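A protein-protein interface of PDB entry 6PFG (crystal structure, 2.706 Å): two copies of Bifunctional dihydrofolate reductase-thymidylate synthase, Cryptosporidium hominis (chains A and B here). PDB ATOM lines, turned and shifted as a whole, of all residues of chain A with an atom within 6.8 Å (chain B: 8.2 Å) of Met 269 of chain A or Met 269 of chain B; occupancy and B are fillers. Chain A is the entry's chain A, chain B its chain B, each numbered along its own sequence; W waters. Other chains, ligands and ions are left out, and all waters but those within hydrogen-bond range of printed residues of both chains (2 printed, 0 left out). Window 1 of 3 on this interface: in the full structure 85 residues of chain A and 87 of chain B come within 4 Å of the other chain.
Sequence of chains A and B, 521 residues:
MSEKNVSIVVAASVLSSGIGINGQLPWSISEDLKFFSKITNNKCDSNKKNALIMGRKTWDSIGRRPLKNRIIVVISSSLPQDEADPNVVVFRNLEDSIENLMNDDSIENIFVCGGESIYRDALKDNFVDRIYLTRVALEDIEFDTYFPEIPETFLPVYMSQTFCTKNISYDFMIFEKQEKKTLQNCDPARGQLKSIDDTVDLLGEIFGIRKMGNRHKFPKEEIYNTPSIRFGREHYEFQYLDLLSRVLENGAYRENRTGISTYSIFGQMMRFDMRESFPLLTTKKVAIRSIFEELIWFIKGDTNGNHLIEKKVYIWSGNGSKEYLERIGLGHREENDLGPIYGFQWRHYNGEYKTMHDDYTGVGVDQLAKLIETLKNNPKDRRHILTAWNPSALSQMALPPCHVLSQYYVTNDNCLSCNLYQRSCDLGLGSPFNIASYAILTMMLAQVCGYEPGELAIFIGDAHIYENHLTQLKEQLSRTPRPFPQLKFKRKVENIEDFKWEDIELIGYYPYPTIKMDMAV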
ATOM      1  N   GLN A 239       1.839 -38.033  17.215  1.00  0.00           N
ATOM      2  CA  GLN A 239       2.019 -36.740  17.869  1.00  0.00           C
ATOM      3  C   GLN A 239       1.064 -35.694  17.309  1.00  0.00           C
ATOM      4  O   GLN A 239       0.691 -34.750  18.016  1.00  0.00           O
ATOM      5  CB  GLN A 239       3.467 -36.281  17.716  1.00  0.00           C
ATOM      6  CG  GLN A 239       4.475 -37.243  18.315  1.00  0.00           C
ATOM      7  CD  GLN A 239       4.701 -37.008  19.792  1.00  0.00           C
ATOM      8  OE1 GLN A 239       4.766 -35.868  20.248  1.00  0.00           O
ATOM      9  NE2 GLN A 239       4.821 -38.090  20.551  1.00  0.00           N
ATOM     10  N   LEU A 243      -2.893 -34.800  19.151  1.00  0.00           N
ATOM     11  CA  LEU A 243      -3.209 -33.389  19.361  1.00  0.00           C
ATOM     12  C   LEU A 243      -4.580 -33.047  18.787  1.00  0.00           C
ATOM     13  O   LEU A 243      -5.352 -32.298  19.402  1.00  0.00           O
ATOM     14  CB  LEU A 243      -2.131 -32.503  18.738  1.00  0.00           C
ATOM     15  CG  LEU A 243      -2.392 -30.994  18.794  1.00  0.00           C
ATOM     16  CD1 LEU A 243      -2.727 -30.551  20.212  1.00  0.00           C
ATOM     17  CD2 LEU A 243      -1.209 -30.210  18.247  1.00  0.00           C
ATOM     18  N   ARG A 246      -6.957 -34.336  21.370  1.00  0.00           N
ATOM     19  CA  ARG A 246      -6.998 -33.485  22.553  1.00  0.00           C
ATOM     20  C   ARG A 246      -7.803 -32.218  22.294  1.00  0.00           C
ATOM     21  O   ARG A 246      -8.566 -31.770  23.159  1.00  0.00           O
ATOM     22  CB  ARG A 246      -5.577 -33.137  22.996  1.00  0.00           C
ATOM     23  CG  ARG A 246      -5.087 -33.926  24.199  1.00  0.00           C
ATOM     24  CD  ARG A 246      -3.745 -34.570  23.907  1.00  0.00           C
ATOM     25  NE  ARG A 246      -2.743 -33.594  23.494  1.00  0.00           N
ATOM     26  CZ  ARG A 246      -1.627 -33.907  22.845  1.00  0.00           C
ATOM     27  NH1 ARG A 246      -1.377 -35.170  22.533  1.00  0.00           N
ATOM     28  NH2 ARG A 246      -0.764 -32.961  22.502  1.00  0.00           N
ATOM     29  N   GLY A 267      -1.151 -24.259  24.547  1.00  0.00           N
ATOM     30  CA  GLY A 267       0.049 -24.896  25.058  1.00  0.00           C
ATOM     31  C   GLY A 267       0.159 -26.381  24.772  1.00  0.00           C
ATOM     32  O   GLY A 267      -0.222 -27.206  25.608  1.00  0.00           O
ATOM     33  N   GLN A 268       0.687 -26.740  23.603  1.00  0.00           N
ATOM     34  CA  GLN A 268       0.853 -28.139  23.229  1.00  0.00           C
ATOM     35  C   GLN A 268       2.202 -28.311  22.547  1.00  0.00           C
ATOM     36  O   GLN A 268       2.891 -27.337  22.245  1.00  0.00           O
ATOM     37  CB  GLN A 268      -0.287 -28.615  22.321  1.00  0.00           C
ATOM     38  CG  GLN A 268      -1.640 -28.658  23.014  1.00  0.00           C
ATOM     39  CD  GLN A 268      -1.732 -29.773  24.037  1.00  0.00           C
ATOM     40  OE1 GLN A 268      -1.297 -30.896  23.783  1.00  0.00           O
ATOM     41  NE2 GLN A 268      -2.290 -29.467  25.202  1.00  0.00           N
ATOM     42  N   MET A 269       2.589 -29.563  22.305  1.00  0.00           N
ATOM     43  CA  MET A 269       3.864 -29.813  21.649  1.00  0.00           C
ATOM     44  C   MET A 269       3.817 -31.128  20.883  1.00  0.00           C
ATOM     45  O   MET A 269       3.032 -32.030  21.191  1.00  0.00           O
ATOM     46  CB  MET A 269       5.024 -29.818  22.651  1.00  0.00           C
ATOM     47  CG  MET A 269       5.256 -31.138  23.360  1.00  0.00           C
ATOM     48  SD  MET A 269       6.900 -31.184  24.104  1.00  0.00           S
ATOM     49  CE  MET A 269       6.876 -32.796  24.886  1.00  0.00           C
ATOM     50  N   MET A 270       4.684 -31.220  19.875  1.00  0.00           N
ATOM     51  CA  MET A 270       4.809 -32.400  19.031  1.00  0.00           C
ATOM     52  C   MET A 270       6.281 -32.667  18.760  1.00  0.00           C
ATOM     53  O   MET A 270       7.040 -31.737  18.474  1.00  0.00           O
ATOM     54  CB  MET A 270       4.069 -32.220  17.697  1.00  0.00           C
ATOM     55  CG  MET A 270       2.560 -32.094  17.807  1.00  0.00           C
ATOM     56  SD  MET A 270       1.763 -31.847  16.201  1.00  0.00           S
ATOM     57  CE  MET A 270       2.431 -30.254  15.723  1.00  0.00           C
ATOM     58  N   ARG A 271       6.681 -33.936  18.840  1.00  0.00           N
ATOM     59  CA  ARG A 271       8.039 -34.354  18.514  1.00  0.00           C
ATOM     60  C   ARG A 271       8.029 -35.235  17.273  1.00  0.00           C
ATOM     61  O   ARG A 271       7.130 -36.059  17.090  1.00  0.00           O
ATOM     62  CB  ARG A 271       8.686 -35.128  19.666  1.00  0.00           C
ATOM     63  CG  ARG A 271       8.566 -34.479  21.027  1.00  0.00           C
ATOM     64  CD  ARG A 271       9.504 -35.156  22.008  1.00  0.00           C
ATOM     65  NE  ARG A 271      10.865 -34.650  21.875  1.00  0.00           N
ATOM     66  CZ  ARG A 271      11.456 -33.862  22.767  1.00  0.00           C
ATOM     67  NH1 ARG A 271      10.812 -33.503  23.869  1.00  0.00           N
ATOM     68  NH2 ARG A 271      12.698 -33.444  22.562  1.00  0.00           N
ATOM     69  N   ALA A 457      10.924 -30.449  17.113  1.00  0.00           N
ATOM     70  CA  ALA A 457       9.921 -30.223  18.144  1.00  0.00           C
ATOM     71  C   ALA A 457       9.162 -28.944  17.824  1.00  0.00           C
ATOM     72  O   ALA A 457       9.772 -27.915  17.512  1.00  0.00           O
ATOM     73  CB  ALA A 457      10.557 -30.140  19.533  1.00  0.00           C
ATOM     74  N   ILE A 458       7.837 -29.019  17.884  1.00  0.00           N
ATOM     75  CA  ILE A 458       6.965 -27.883  17.611  1.00  0.00           C
ATOM     76  C   ILE A 458       6.176 -27.586  18.876  1.00  0.00           C
ATOM     77  O   ILE A 458       5.455 -28.455  19.383  1.00  0.00           O
ATOM     78  CB  ILE A 458       6.026 -28.158  16.429  1.00  0.00           C
ATOM     79  CG1 ILE A 458       6.840 -28.411  15.157  1.00  0.00           C
ATOM     80  CG2 ILE A 458       5.053 -27.002  16.242  1.00  0.00           C
ATOM     81  CD1 ILE A 458       5.997 -28.693  13.939  1.00  0.00           C
ATOM     82  N   PHE A 459       6.328 -26.368  19.393  1.00  0.00           N
ATOM     83  CA  PHE A 459       5.595 -25.894  20.558  1.00  0.00           C
ATOM     84  C   PHE A 459       4.546 -24.891  20.098  1.00  0.00           C
ATOM     85  O   PHE A 459       4.863 -23.945  19.370  1.00  0.00           O
ATOM     86  CB  PHE A 459       6.536 -25.259  21.582  1.00  0.00           C
ATOM     87  CG  PHE A 459       7.700 -26.133  21.957  1.00  0.00           C
ATOM     88  CD1 PHE A 459       7.497 -27.331  22.621  1.00  0.00           C
ATOM     89  CD2 PHE A 459       8.996 -25.755  21.651  1.00  0.00           C
ATOM     90  CE1 PHE A 459       8.566 -28.140  22.970  1.00  0.00           C
ATOM     91  CE2 PHE A 459      10.071 -26.559  21.996  1.00  0.00           C
ATOM     92  CZ  PHE A 459       9.855 -27.753  22.657  1.00  0.00           C
ATOM     93  N   ILE A 460       3.303 -25.102  20.519  1.00  0.00           N
ATOM     94  CA  ILE A 460       2.148 -24.408  19.966  1.00  0.00           C
ATOM     95  C   ILE A 460       1.433 -23.661  21.082  1.00  0.00           C
ATOM     96  O   ILE A 460       1.185 -24.224  22.157  1.00  0.00           O
ATOM     97  CB  ILE A 460       1.183 -25.387  19.278  1.00  0.00           C
ATOM     98  CG1 ILE A 460       1.889 -26.116  18.133  1.00  0.00           C
ATOM     99  CG2 ILE A 460      -0.042 -24.648  18.782  1.00  0.00           C
ATOM    100  CD1 ILE A 460       1.038 -27.177  17.476  1.00  0.00           C
ATOM    101  N   PHE B 238       6.938 -31.990  40.075  1.00  0.00           N
ATOM    102  CA  PHE B 238       7.572 -33.080  39.346  1.00  0.00           C
ATOM    103  C   PHE B 238       7.919 -32.689  37.916  1.00  0.00           C
ATOM    104  O   PHE B 238       8.794 -33.316  37.314  1.00  0.00           O
ATOM    105  CB  PHE B 238       6.660 -34.309  39.346  1.00  0.00           C
ATOM    106  CG  PHE B 238       6.592 -35.013  40.672  1.00  0.00           C
ATOM    107  CD1 PHE B 238       7.751 -35.412  41.320  1.00  0.00           C
ATOM    108  CD2 PHE B 238       5.368 -35.259  41.279  1.00  0.00           C
ATOM    109  CE1 PHE B 238       7.690 -36.057  42.541  1.00  0.00           C
ATOM    110  CE2 PHE B 238       5.301 -35.900  42.505  1.00  0.00           C
ATOM    111  CZ  PHE B 238       6.462 -36.300  43.136  1.00  0.00           C
ATOM    112  N   GLN B 239       7.264 -31.665  37.362  1.00  0.00           N
ATOM    113  CA  GLN B 239       7.610 -31.210  36.019  1.00  0.00           C
ATOM    114  C   GLN B 239       9.032 -30.666  35.958  1.00  0.00           C
ATOM    115  O   GLN B 239       9.669 -30.712  34.900  1.00  0.00           O
ATOM    116  CB  GLN B 239       6.614 -30.150  35.552  1.00  0.00           C
ATOM    117  CG  GLN B 239       5.176 -30.635  35.484  1.00  0.00           C
ATOM    118  CD  GLN B 239       4.848 -31.308  34.166  1.00  0.00           C
ATOM    119  OE1 GLN B 239       5.279 -30.861  33.104  1.00  0.00           O
ATOM    120  NE2 GLN B 239       4.079 -32.389  34.227  1.00  0.00           N
ATOM    121  N   TYR B 240       9.545 -30.156  37.077  1.00  0.00           N
ATOM    122  CA  TYR B 240      10.910 -29.649  37.162  1.00  0.00           C
ATOM    123  C   TYR B 240      11.898 -30.738  37.567  1.00  0.00           C
ATOM    124  O   TYR B 240      12.977 -30.866  36.970  1.00  0.00           O
ATOM    125  CB  TYR B 240      10.961 -28.477  38.152  1.00  0.00           C
ATOM    126  CG  TYR B 240      12.356 -28.040  38.521  1.00  0.00           C
ATOM    127  CD1 TYR B 240      13.089 -27.208  37.686  1.00  0.00           C
ATOM    128  CD2 TYR B 240      12.944 -28.460  39.709  1.00  0.00           C
ATOM    129  CE1 TYR B 240      14.372 -26.812  38.021  1.00  0.00           C
ATOM    130  CE2 TYR B 240      14.224 -28.068  40.051  1.00  0.00           C
ATOM    131  CZ  TYR B 240      14.933 -27.244  39.203  1.00  0.00           C
ATOM    132  OH  TYR B 240      16.207 -26.852  39.542  1.00  0.00           O
ATOM    133  N   ASP B 242      11.578 -33.994  37.230  1.00  0.00           N
ATOM    134  CA  ASP B 242      11.708 -34.980  36.166  1.00  0.00           C
ATOM    135  C   ASP B 242      12.530 -34.444  35.000  1.00  0.00           C
ATOM    136  O   ASP B 242      13.218 -35.217  34.329  1.00  0.00           O
ATOM    137  CB  ASP B 242      10.327 -35.433  35.692  1.00  0.00           C
ATOM    138  CG  ASP B 242       9.562 -36.191  36.765  1.00  0.00           C
ATOM    139  OD1 ASP B 242      10.123 -36.394  37.863  1.00  0.00           O
ATOM    140  OD2 ASP B 242       8.408 -36.596  36.506  1.00  0.00           O
ATOM    141  N   LEU B 243      12.486 -33.134  34.747  1.00  0.00           N
ATOM    142  CA  LEU B 243      13.376 -32.558  33.743  1.00  0.00           C
ATOM    143  C   LEU B 243      14.830 -32.625  34.199  1.00  0.00           C
ATOM    144  O   LEU B 243      15.723 -32.939  33.401  1.00  0.00           O
ATOM    145  CB  LEU B 243      12.965 -31.117  33.438  1.00  0.00           C
ATOM    146  CG  LEU B 243      13.858 -30.331  32.476  1.00  0.00           C
ATOM    147  CD1 LEU B 243      14.101 -31.119  31.204  1.00  0.00           C
ATOM    148  CD2 LEU B 243      13.230 -28.984  32.156  1.00  0.00           C
ATOM    149  N   ARG B 246      15.789 -36.183  33.563  1.00  0.00           N
ATOM    150  CA  ARG B 246      16.000 -36.444  32.145  1.00  0.00           C
ATOM    151  C   ARG B 246      17.342 -35.897  31.684  1.00  0.00           C
ATOM    152  O   ARG B 246      18.040 -36.534  30.888  1.00  0.00           O
ATOM    153  CB  ARG B 246      14.860 -35.844  31.324  1.00  0.00           C
ATOM    154  CG  ARG B 246      13.848 -36.867  30.833  1.00  0.00           C
ATOM    155  CD  ARG B 246      12.433 -36.462  31.195  1.00  0.00           C
ATOM    156  NE  ARG B 246      12.075 -35.142  30.683  1.00  0.00           N
ATOM    157  CZ  ARG B 246      11.069 -34.414  31.159  1.00  0.00           C
ATOM    158  NH1 ARG B 246      10.336 -34.877  32.161  1.00  0.00           N
ATOM    159  NH2 ARG B 246      10.799 -33.223  30.642  1.00  0.00           N
ATOM    160  N   ILE B 265      20.351 -31.210  26.989  1.00  0.00           N
ATOM    161  CA  ILE B 265      19.420 -31.799  26.036  1.00  0.00           C
ATOM    162  C   ILE B 265      18.636 -30.668  25.378  1.00  0.00           C
ATOM    163  O   ILE B 265      18.681 -29.514  25.812  1.00  0.00           O
ATOM    164  CB  ILE B 265      18.467 -32.827  26.682  1.00  0.00           C
ATOM    165  CG1 ILE B 265      17.620 -32.178  27.777  1.00  0.00           C
ATOM    166  CG2 ILE B 265      19.243 -34.014  27.231  1.00  0.00           C
ATOM    167  CD1 ILE B 265      16.616 -33.124  28.396  1.00  0.00           C
ATOM    168  N   PHE B 266      17.916 -31.010  24.311  1.00  0.00           N
ATOM    169  CA  PHE B 266      17.260 -30.019  23.469  1.00  0.00           C
ATOM    170  C   PHE B 266      15.787 -30.362  23.292  1.00  0.00           C
ATOM    171  O   PHE B 266      15.453 -31.472  22.864  1.00  0.00           O
ATOM    172  CB  PHE B 266      17.951 -29.923  22.103  1.00  0.00           C
ATOM    173  CG  PHE B 266      17.478 -28.771  21.263  1.00  0.00           C
ATOM    174  CD1 PHE B 266      17.718 -27.464  21.657  1.00  0.00           C
ATOM    175  CD2 PHE B 266      16.801 -28.994  20.076  1.00  0.00           C
ATOM    176  CE1 PHE B 266      17.290 -26.402  20.884  1.00  0.00           C
ATOM    177  CE2 PHE B 266      16.369 -27.934  19.297  1.00  0.00           C
ATOM    178  CZ  PHE B 266      16.614 -26.637  19.701  1.00  0.00           C
ATOM    179  N   GLY B 267      14.916 -29.402  23.609  1.00  0.00           N
ATOM    180  CA  GLY B 267      13.482 -29.542  23.410  1.00  0.00           C
ATOM    181  C   GLY B 267      12.739 -30.186  24.564  1.00  0.00           C
ATOM    182  O   GLY B 267      12.504 -31.399  24.553  1.00  0.00           O
ATOM    183  N   GLN B 268      12.340 -29.389  25.557  1.00  0.00           N
ATOM    184  CA  GLN B 268      11.620 -29.901  26.717  1.00  0.00           C
ATOM    185  C   GLN B 268      10.499 -28.936  27.080  1.00  0.00           C
ATOM    186  O   GLN B 268      10.400 -27.838  26.531  1.00  0.00           O
ATOM    187  CB  GLN B 268      12.557 -30.115  27.912  1.00  0.00           C
ATOM    188  CG  GLN B 268      13.587 -31.211  27.690  1.00  0.00           C
ATOM    189  CD  GLN B 268      12.970 -32.593  27.660  1.00  0.00           C
ATOM    190  OE1 GLN B 268      12.108 -32.922  28.476  1.00  0.00           O
ATOM    191  NE2 GLN B 268      13.402 -33.412  26.710  1.00  0.00           N
ATOM    192  N   MET B 269       9.642 -29.352  28.014  1.00  0.00           N
ATOM    193  CA  MET B 269       8.544 -28.491  28.433  1.00  0.00           C
ATOM    194  C   MET B 269       8.136 -28.806  29.866  1.00  0.00           C
ATOM    195  O   MET B 269       8.363 -29.905  30.379  1.00  0.00           O
ATOM    196  CB  MET B 269       7.337 -28.621  27.497  1.00  0.00           C
ATOM    197  CG  MET B 269       6.414 -29.779  27.808  1.00  0.00           C
ATOM    198  SD  MET B 269       4.815 -29.589  26.997  1.00  0.00           S
ATOM    199  CE  MET B 269       3.992 -31.094  27.513  1.00  0.00           C
ATOM    200  N   MET B 270       7.528 -27.807  30.505  1.00  0.00           N
ATOM    201  CA  MET B 270       7.024 -27.911  31.867  1.00  0.00           C
ATOM    202  C   MET B 270       5.677 -27.212  31.960  1.00  0.00           C
ATOM    203  O   MET B 270       5.504 -26.119  31.417  1.00  0.00           O
ATOM    204  CB  MET B 270       7.994 -27.286  32.881  1.00  0.00           C
ATOM    205  CG  MET B 270       9.319 -28.008  33.021  1.00  0.00           C
ATOM    206  SD  MET B 270      10.413 -27.204  34.210  1.00  0.00           S
ATOM    207  CE  MET B 270      10.708 -25.633  33.400  1.00  0.00           C
ATOM    208  N   ARG B 271       4.724 -27.841  32.646  1.00  0.00           N
ATOM    209  CA  ARG B 271       3.419 -27.245  32.904  1.00  0.00           C
ATOM    210  C   ARG B 271       3.245 -26.996  34.396  1.00  0.00           C
ATOM    211  O   ARG B 271       3.689 -27.795  35.225  1.00  0.00           O
ATOM    212  CB  ARG B 271       2.273 -28.135  32.414  1.00  0.00           C
ATOM    213  CG  ARG B 271       2.416 -28.679  31.008  1.00  0.00           C
ATOM    214  CD  ARG B 271       1.081 -29.235  30.536  1.00  0.00           C
ATOM    215  NE  ARG B 271       0.222 -28.172  30.026  1.00  0.00           N
ATOM    216  CZ  ARG B 271      -0.072 -28.008  28.740  1.00  0.00           C
ATOM    217  NH1 ARG B 271       0.405 -28.854  27.835  1.00  0.00           N
ATOM    218  NH2 ARG B 271      -0.853 -27.007  28.357  1.00  0.00           N
ATOM    219  N   PHE B 272       2.587 -25.891  34.733  1.00  0.00           N
ATOM    220  CA  PHE B 272       2.294 -25.556  36.118  1.00  0.00           C
ATOM    221  C   PHE B 272       0.900 -24.956  36.202  1.00  0.00           C
ATOM    222  O   PHE B 272       0.516 -24.136  35.363  1.00  0.00           O
ATOM    223  CB  PHE B 272       3.323 -24.571  36.686  1.00  0.00           C
ATOM    224  CG  PHE B 272       4.734 -25.081  36.649  1.00  0.00           C
ATOM    225  CD1 PHE B 272       5.216 -25.900  37.658  1.00  0.00           C
ATOM    226  CD2 PHE B 272       5.578 -24.744  35.604  1.00  0.00           C
ATOM    227  CE1 PHE B 272       6.514 -26.370  37.627  1.00  0.00           C
ATOM    228  CE2 PHE B 272       6.880 -25.213  35.566  1.00  0.00           C
ATOM    229  CZ  PHE B 272       7.348 -26.027  36.577  1.00  0.00           C
ATOM    230  N   ASN B 419       2.381 -18.960  27.898  1.00  0.00           N
ATOM    231  CA  ASN B 419       3.393 -19.837  27.327  1.00  0.00           C
ATOM    232  C   ASN B 419       4.693 -19.056  27.201  1.00  0.00           C
ATOM    233  O   ASN B 419       4.680 -17.880  26.828  1.00  0.00           O
ATOM    234  CB  ASN B 419       2.972 -20.362  25.951  1.00  0.00           C
ATOM    235  CG  ASN B 419       1.925 -21.451  26.036  1.00  0.00           C
ATOM    236  OD1 ASN B 419       1.535 -21.870  27.124  1.00  0.00           O
ATOM    237  ND2 ASN B 419       1.451 -21.905  24.881  1.00  0.00           N
ATOM    238  N   LEU B 420       5.811 -19.705  27.509  1.00  0.00           N
ATOM    239  CA  LEU B 420       7.122 -19.073  27.424  1.00  0.00           C
ATOM    240  C   LEU B 420       8.073 -19.989  26.671  1.00  0.00           C
ATOM    241  O   LEU B 420       8.257 -21.146  27.059  1.00  0.00           O
ATOM    242  CB  LEU B 420       7.676 -18.763  28.818  1.00  0.00           C
ATOM    243  CG  LEU B 420       9.166 -18.417  28.877  1.00  0.00           C
ATOM    244  CD1 LEU B 420       9.439 -17.083  28.221  1.00  0.00           C
ATOM    245  CD2 LEU B 420       9.664 -18.416  30.313  1.00  0.00           C
ATOM    246  N   LEU B 456       0.669 -22.086  33.321  1.00  0.00           N
ATOM    247  CA  LEU B 456       1.969 -21.615  32.860  1.00  0.00           C
ATOM    248  C   LEU B 456       2.688 -22.770  32.182  1.00  0.00           C
ATOM    249  O   LEU B 456       2.972 -23.786  32.821  1.00  0.00           O
ATOM    250  CB  LEU B 456       2.808 -21.068  34.018  1.00  0.00           C
ATOM    251  CG  LEU B 456       4.252 -20.692  33.678  1.00  0.00           C
ATOM    252  CD1 LEU B 456       4.277 -19.552  32.671  1.00  0.00           C
ATOM    253  CD2 LEU B 456       5.032 -20.321  34.932  1.00  0.00           C
ATOM    254  N   ALA B 457       2.976 -22.618  30.894  1.00  0.00           N
ATOM    255  CA  ALA B 457       3.739 -23.603  30.141  1.00  0.00           C
ATOM    256  C   ALA B 457       5.063 -22.988  29.713  1.00  0.00           C
ATOM    257  O   ALA B 457       5.096 -21.868  29.190  1.00  0.00           O
ATOM    258  CB  ALA B 457       2.955 -24.097  28.923  1.00  0.00           C
ATOM    259  N   ILE B 458       6.153 -23.713  29.951  1.00  0.00           N
ATOM    260  CA  ILE B 458       7.496 -23.268  29.600  1.00  0.00           C
ATOM    261  C   ILE B 458       8.077 -24.265  28.610  1.00  0.00           C
ATOM    262  O   ILE B 458       8.186 -25.459  28.915  1.00  0.00           O
ATOM    263  CB  ILE B 458       8.397 -23.134  30.837  1.00  0.00           C
ATOM    264  CG1 ILE B 458       7.820 -22.097  31.804  1.00  0.00           C
ATOM    265  CG2 ILE B 458       9.814 -22.758  30.427  1.00  0.00           C
ATOM    266  CD1 ILE B 458       8.643 -21.898  33.052  1.00  0.00           C
ATOM    267  N   PHE B 459       8.436 -23.778  27.425  1.00  0.00           N
ATOM    268  CA  PHE B 459       9.072 -24.577  26.389  1.00  0.00           C
ATOM    269  C   PHE B 459      10.539 -24.182  26.298  1.00  0.00           C
ATOM    270  O   PHE B 459      10.861 -22.996  26.174  1.00  0.00           O
ATOM    271  CB  PHE B 459       8.371 -24.379  25.043  1.00  0.00           C
ATOM    272  CG  PHE B 459       6.885 -24.587  25.103  1.00  0.00           C
ATOM    273  CD1 PHE B 459       6.358 -25.837  25.388  1.00  0.00           C
ATOM    274  CD2 PHE B 459       6.016 -23.533  24.882  1.00  0.00           C
ATOM    275  CE1 PHE B 459       4.991 -26.034  25.446  1.00  0.00           C
ATOM    276  CE2 PHE B 459       4.644 -23.720  24.940  1.00  0.00           C
ATOM    277  CZ  PHE B 459       4.130 -24.973  25.222  1.00  0.00           C
ATOM    278  N   ILE B 460      11.424 -25.173  26.355  1.00  0.00           N
ATOM    279  CA  ILE B 460      12.851 -24.956  26.550  1.00  0.00           C
ATOM    280  C   ILE B 460      13.615 -25.553  25.379  1.00  0.00           C
ATOM    281  O   ILE B 460      13.342 -26.687  24.963  1.00  0.00           O
ATOM    282  CB  ILE B 460      13.337 -25.570  27.874  1.00  0.00           C
ATOM    283  CG1 ILE B 460      12.611 -24.933  29.059  1.00  0.00           C
ATOM    284  CG2 ILE B 460      14.839 -25.412  28.003  1.00  0.00           C
ATOM    285  CD1 ILE B 460      12.960 -25.555  30.392  1.00  0.00           C
ATOM    286  N   GLY B 461      14.574 -24.789  24.858  1.00  0.00           N
ATOM    287  CA  GLY B 461      15.522 -25.294  23.888  1.00  0.00           C
ATOM    288  C   GLY B 461      16.641 -26.074  24.550  1.00  0.00           C
ATOM    289  O   GLY B 461      16.512 -27.281  24.770  1.00  0.00           O
ATOM    290  N   ALA B 463      18.179 -27.183  27.490  1.00  0.00           N
ATOM    291  CA  ALA B 463      18.030 -27.387  28.926  1.00  0.00           C
ATOM    292  C   ALA B 463      19.276 -28.093  29.443  1.00  0.00           C
ATOM    293  O   ALA B 463      19.593 -29.203  28.995  1.00  0.00           O
ATOM    294  CB  ALA B 463      16.776 -28.204  29.232  1.00  0.00           C
HETATM  295  O   HOH W   1      -3.235 -27.247  26.581  1.00  0.00           O
HETATM  296  O   HOH W   2      14.710 -33.155  24.407  1.00  0.00           O
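Of the printed residues of chain B, Gly 267 of chain A touches Arg 271 and Asn 419.
Met 269 of chain A touches just one residue of chain B: Met 269 (3.9 Å).
Of the printed residues of chain B, Phe 459 of chain A touches Gln 268 and Phe 459.
Phe 238 of chain B touches none of the printed residues of chain A.
Printed residues of chain A within 4 Å of Arg 271 of chain B: Gly 267 and Gln 268.
Of the printed residues of chain A, Phe 459 of chain B touches Gln 268 and Phe 459.
The nearest residue of chain B that does not touch Met 269 of chain A is Phe 459 of chain B (4.7 Å).
The nearest residue of chain A that does not touch Met 269 of chain B is Phe 459 of chain A (4.7 Å).
Hydrophobic or aromatic side chains of chain A within 4 Å of the printed part of chain B: Met 269 and Phe 459.
Among the printed residues, 11 pairs touch across the chains.
Among the printed residues, no Asp or Glu carboxylate lies within 4 Å of a Lys or Arg side-chain nitrogen of the other chain.
Met 269 of chain B touches its own counterpart, Met 269 of chain A.
Phe 459 of chain A touches its own counterpart, Phe 459 of chain B.
Positions printed for both chains: 239, 243, 246, 267, 268, 269, 270, 271, 457, 458, 459 and 460.
Of the 11 pairs that touch across the chains among the printed residues, 8 have their exchanged pair printed and touching as well.
Among the printed residues, pairs that only touch across the chains: Gly 267 of chain A with Asn 419 of chain B, Phe 459 of chain A with Phe 459 of chain B, Ile 460 of chain A with Asn 419 of chain B, Gln 268 of chain A with Arg 271 of chain B, Arg 271 of chain A with Gln 268 of chain B, Met 269 of chain A with Met 269 of chain B, Phe 459 of chain A with Gln 268 of chain B and Gln 268 of chain A with Phe 459 of chain B.
The backbone carbonyl oxygen (O) of Gly 267 of chain A is in hydrogen-bond range of the guanidinium group (NH2) of Arg 271 of chain B, at 2.8 Å.
The backbone carbonyl oxygen (O) of Phe 266 of chain B is in hydrogen-bond range of the guanidinium group (NH2) of Arg 271 of chain A (3.4 Å).
NH1 of Arg 271 of chain A sits at hydrogen-bond distance from O of Gly 267 of chain B (2.8 Å).
Water W1 lies within hydrogen-bond range of the side-chain amide nitrogen (NE2) of Gln 268 of chain A, the guanidinium group (NH2) of Arg 271 of chain B and the backbone carbonyl oxygen (O) of Gly 267 of chain A.
The side-chain amide oxygen (OE1) of Gln 268 of chain A is in hydrogen-bond range of the guanidinium group (NH2) of Arg 246 of chain A (2.5 Å).
The backbone NH of Arg 271 of chain B sits at hydrogen-bond distance from the side-chain amide oxygen of Gln 239 of chain B (3.1 Å).
N of Gly 267 of chain B is in hydrogen-bond range of O of Gly 461 of chain B, 2.9 Å away.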
